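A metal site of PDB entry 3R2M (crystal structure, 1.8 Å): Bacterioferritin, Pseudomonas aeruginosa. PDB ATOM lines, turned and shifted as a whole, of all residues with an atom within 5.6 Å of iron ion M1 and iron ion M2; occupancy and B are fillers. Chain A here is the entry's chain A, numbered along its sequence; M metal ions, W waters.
OH of Tyr 25 lies close to OE2 of Glu 93 (2.6 Å). OE1 of Glu 50 is in hydrogen-bond range of NE2 of His 130. The backbone carbonyl oxygen (O) of His 54 is in hydrogen-bond range of the side-chain amide nitrogen (NE2) of Gln 122, 3.1 Å away.
Three residues have an atom within 4 Å of iron ion M1: Glu 18, Glu 51 and His 54. The nearest printed residue that does not touch iron ion M1 is Thr 126 (4.2 Å).
Of the 12 residues printed, 3 come within 4 Å of iron ion M2. The nearest printed residue that does not touch iron ion M2 is Thr 126 (4.1 Å).
Iron ion M1 is bound by water W2 (2.1 Å), OE1 of Glu 18 (2.1 Å), water W1 (2.2 Å), OE1 of Glu 51 (2.2 Å) and ND1 of His 54 (2.3 Å). Iron ion M1 has five donor atoms within binding distance.
Iron ion M2 is bound by water W2, 2.0 Å away. Iron ion M2 is bound by OE2 of Glu 51. The side-chain carboxylate (OE2) of Glu 93 binds iron ion M2 (2.2 Å). ND1 of His 130 is bound to iron ion M2. OE1 of Glu 93 binds iron ion M2 (2.3 Å).
Water W1 bridges OE2 of Glu 18 (2.7 Å) and OE1 of Gln 122 (3.2 Å).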
ATOM      1  N   GLU A  18       2.314  15.469  -3.984  1.00  0.00           N
ATOM      2  CA  GLU A  18       2.628  14.931  -5.323  1.00  0.00           C
ATOM      3  C   GLU A  18       2.919  13.445  -5.256  1.00  0.00           C
ATOM      4  O   GLU A  18       2.541  12.680  -6.145  1.00  0.00           O
ATOM      5  CB  GLU A  18       3.845  15.664  -5.939  1.00  0.00           C
ATOM      6  CG  GLU A  18       3.637  17.142  -6.156  1.00  0.00           C
ATOM      7  CD  GLU A  18       2.484  17.450  -7.065  1.00  0.00           C
ATOM      8  OE1 GLU A  18       2.341  16.766  -8.088  1.00  0.00           O
ATOM      9  OE2 GLU A  18       1.709  18.371  -6.765  1.00  0.00           O
ATOM     10  N   ALA A  21      -0.471  11.925  -5.153  1.00  0.00           N
ATOM     11  CA  ALA A  21      -1.116  11.961  -6.487  1.00  0.00           C
ATOM     12  C   ALA A  21      -0.564  10.824  -7.368  1.00  0.00           C
ATOM     13  O   ALA A  21      -1.332  10.092  -8.007  1.00  0.00           O
ATOM     14  CB  ALA A  21      -0.854  13.301  -7.160  1.00  0.00           C
ATOM     15  N   TYR A  25      -2.888   7.674  -8.794  1.00  0.00           N
ATOM     16  CA  TYR A  25      -2.946   7.302 -10.207  1.00  0.00           C
ATOM     17  C   TYR A  25      -2.365   5.894 -10.435  1.00  0.00           C
ATOM     18  O   TYR A  25      -2.817   5.194 -11.340  1.00  0.00           O
ATOM     19  CB  TYR A  25      -2.154   8.325 -11.032  1.00  0.00           C
ATOM     20  CG  TYR A  25      -2.857   9.660 -11.195  1.00  0.00           C
ATOM     21  CD1 TYR A  25      -4.204   9.717 -11.546  1.00  0.00           C
ATOM     22  CD2 TYR A  25      -2.166  10.856 -11.053  1.00  0.00           C
ATOM     23  CE1 TYR A  25      -4.854  10.931 -11.742  1.00  0.00           C
ATOM     24  CE2 TYR A  25      -2.813  12.074 -11.218  1.00  0.00           C
ATOM     25  CZ  TYR A  25      -4.163  12.100 -11.576  1.00  0.00           C
ATOM     26  OH  TYR A  25      -4.826  13.291 -11.797  1.00  0.00           O
ATOM     27  N   GLU A  50       3.878  11.613 -14.802  1.00  0.00           N
ATOM     28  CA  GLU A  50       3.954  13.068 -14.662  1.00  0.00           C
ATOM     29  C   GLU A  50       4.000  13.555 -13.201  1.00  0.00           C
ATOM     30  O   GLU A  50       4.748  14.479 -12.876  1.00  0.00           O
ATOM     31  CB  GLU A  50       2.802  13.743 -15.402  1.00  0.00           C
ATOM     32  CG  GLU A  50       2.905  13.581 -16.917  1.00  0.00           C
ATOM     33  CD  GLU A  50       1.973  14.477 -17.678  1.00  0.00           C
ATOM     34  OE1 GLU A  50       0.864  14.754 -17.187  1.00  0.00           O
ATOM     35  OE2 GLU A  50       2.347  14.930 -18.782  1.00  0.00           O
ATOM     36  N   GLU A  51       3.208  12.939 -12.323  1.00  0.00           N
ATOM     37  CA  GLU A  51       3.288  13.313 -10.910  1.00  0.00           C
ATOM     38  C   GLU A  51       4.626  12.884 -10.332  1.00  0.00           C
ATOM     39  O   GLU A  51       5.139  13.545  -9.440  1.00  0.00           O
ATOM     40  CB  GLU A  51       2.185  12.655 -10.078  1.00  0.00           C
ATOM     41  CG  GLU A  51       0.788  12.920 -10.552  1.00  0.00           C
ATOM     42  CD  GLU A  51       0.380  14.390 -10.516  1.00  0.00           C
ATOM     43  OE1 GLU A  51       1.154  15.225 -10.071  1.00  0.00           O
ATOM     44  OE2 GLU A  51      -0.746  14.684 -10.934  1.00  0.00           O
ATOM     45  N   HIS A  54       6.766  15.632 -11.227  1.00  0.00           N
ATOM     46  CA  HIS A  54       6.455  16.798 -10.376  1.00  0.00           C
ATOM     47  C   HIS A  54       7.097  16.656  -9.005  1.00  0.00           C
ATOM     48  O   HIS A  54       7.708  17.569  -8.502  1.00  0.00           O
ATOM     49  CB  HIS A  54       4.935  16.954 -10.208  1.00  0.00           C
ATOM     50  CG  HIS A  54       4.252  17.512 -11.406  1.00  0.00           C
ATOM     51  ND1 HIS A  54       2.895  17.675 -11.475  1.00  0.00           N
ATOM     52  CD2 HIS A  54       4.739  17.953 -12.596  1.00  0.00           C
ATOM     53  CE1 HIS A  54       2.563  18.185 -12.635  1.00  0.00           C
ATOM     54  NE2 HIS A  54       3.667  18.372 -13.334  1.00  0.00           N
ATOM     55  N   GLU A  93      -6.792  16.866  -7.818  1.00  0.00           N
ATOM     56  CA  GLU A  93      -6.152  17.889  -8.658  1.00  0.00           C
ATOM     57  C   GLU A  93      -6.605  19.289  -8.257  1.00  0.00           C
ATOM     58  O   GLU A  93      -5.818  20.232  -8.311  1.00  0.00           O
ATOM     59  CB  GLU A  93      -6.476  17.657 -10.138  1.00  0.00           C
ATOM     60  CG  GLU A  93      -5.835  16.356 -10.675  1.00  0.00           C
ATOM     61  CD  GLU A  93      -4.304  16.493 -10.837  1.00  0.00           C
ATOM     62  OE1 GLU A  93      -3.800  17.626 -10.944  1.00  0.00           O
ATOM     63  OE2 GLU A  93      -3.628  15.447 -10.907  1.00  0.00           O
ATOM     64  N   VAL A  96      -4.509  20.126  -5.257  1.00  0.00           N
ATOM     65  CA  VAL A  96      -3.184  20.485  -5.748  1.00  0.00           C
ATOM     66  C   VAL A  96      -3.163  21.885  -6.390  1.00  0.00           C
ATOM     67  O   VAL A  96      -2.256  22.684  -6.106  1.00  0.00           O
ATOM     68  CB  VAL A  96      -2.653  19.425  -6.762  1.00  0.00           C
ATOM     69  CG1 VAL A  96      -1.357  19.949  -7.403  1.00  0.00           C
ATOM     70  CG2 VAL A  96      -2.392  18.109  -6.020  1.00  0.00           C
ATOM     71  N   LEU A 100      -0.757  24.784  -5.008  1.00  0.00           N
ATOM     72  CA  LEU A 100       0.277  25.387  -5.844  1.00  0.00           C
ATOM     73  C   LEU A 100       0.084  26.896  -5.938  1.00  0.00           C
ATOM     74  O   LEU A 100       1.054  27.656  -5.892  1.00  0.00           O
ATOM     75  CB  LEU A 100       0.252  24.754  -7.265  1.00  0.00           C
ATOM     76  CG  LEU A 100       0.819  23.327  -7.361  1.00  0.00           C
ATOM     77  CD1 LEU A 100       0.420  22.721  -8.705  1.00  0.00           C
ATOM     78  CD2 LEU A 100       2.356  23.355  -7.190  1.00  0.00           C
ATOM     79  N   GLN A 122       4.132  23.525 -12.776  1.00  0.00           N
ATOM     80  CA  GLN A 122       3.243  22.486 -12.293  1.00  0.00           C
ATOM     81  C   GLN A 122       1.786  22.905 -12.242  1.00  0.00           C
ATOM     82  O   GLN A 122       0.884  22.092 -12.472  1.00  0.00           O
ATOM     83  CB  GLN A 122       3.715  21.991 -10.933  1.00  0.00           C
ATOM     84  CG  GLN A 122       5.081  21.353 -11.015  1.00  0.00           C
ATOM     85  CD  GLN A 122       5.451  20.624  -9.735  1.00  0.00           C
ATOM     86  OE1 GLN A 122       4.609  20.355  -8.885  1.00  0.00           O
ATOM     87  NE2 GLN A 122       6.719  20.260  -9.623  1.00  0.00           N
ATOM     88  N   THR A 126      -1.326  21.042 -13.986  1.00  0.00           N
ATOM     89  CA  THR A 126      -2.498  20.681 -13.178  1.00  0.00           C
ATOM     90  C   THR A 126      -3.819  21.208 -13.786  1.00  0.00           C
ATOM     91  O   THR A 126      -4.808  20.482 -13.894  1.00  0.00           O
ATOM     92  CB  THR A 126      -2.303  21.233 -11.751  1.00  0.00           C
ATOM     93  OG1 THR A 126      -1.147  20.604 -11.163  1.00  0.00           O
ATOM     94  CG2 THR A 126      -3.546  21.002 -10.902  1.00  0.00           C
ATOM     95  N   HIS A 130      -4.121  17.867 -16.409  1.00  0.00           N
ATOM     96  CA  HIS A 130      -4.715  16.894 -15.474  1.00  0.00           C
ATOM     97  C   HIS A 130      -6.177  17.181 -15.115  1.00  0.00           C
ATOM     98  O   HIS A 130      -7.051  16.340 -15.333  1.00  0.00           O
ATOM     99  CB  HIS A 130      -3.898  16.843 -14.198  1.00  0.00           C
ATOM    100  CG  HIS A 130      -2.456  16.478 -14.416  1.00  0.00           C
ATOM    101  ND1 HIS A 130      -1.541  16.398 -13.396  1.00  0.00           N
ATOM    102  CD2 HIS A 130      -1.781  16.169 -15.553  1.00  0.00           C
ATOM    103  CE1 HIS A 130      -0.361  16.065 -13.881  1.00  0.00           C
ATOM    104  NE2 HIS A 130      -0.481  15.920 -15.190  1.00  0.00           N
HETATM  105 FE    FE M   1       1.279  17.395  -9.837  1.00  0.00          FE
HETATM  106 FE    FE M   2      -1.752  16.499 -11.163  1.00  0.00          FE
HETATM  107  O   HOH W   1       1.517  19.458  -9.188  1.00  0.00           O
HETATM  108  O   HOH W   2      -0.563  17.989 -10.627  1.00  0.00           O
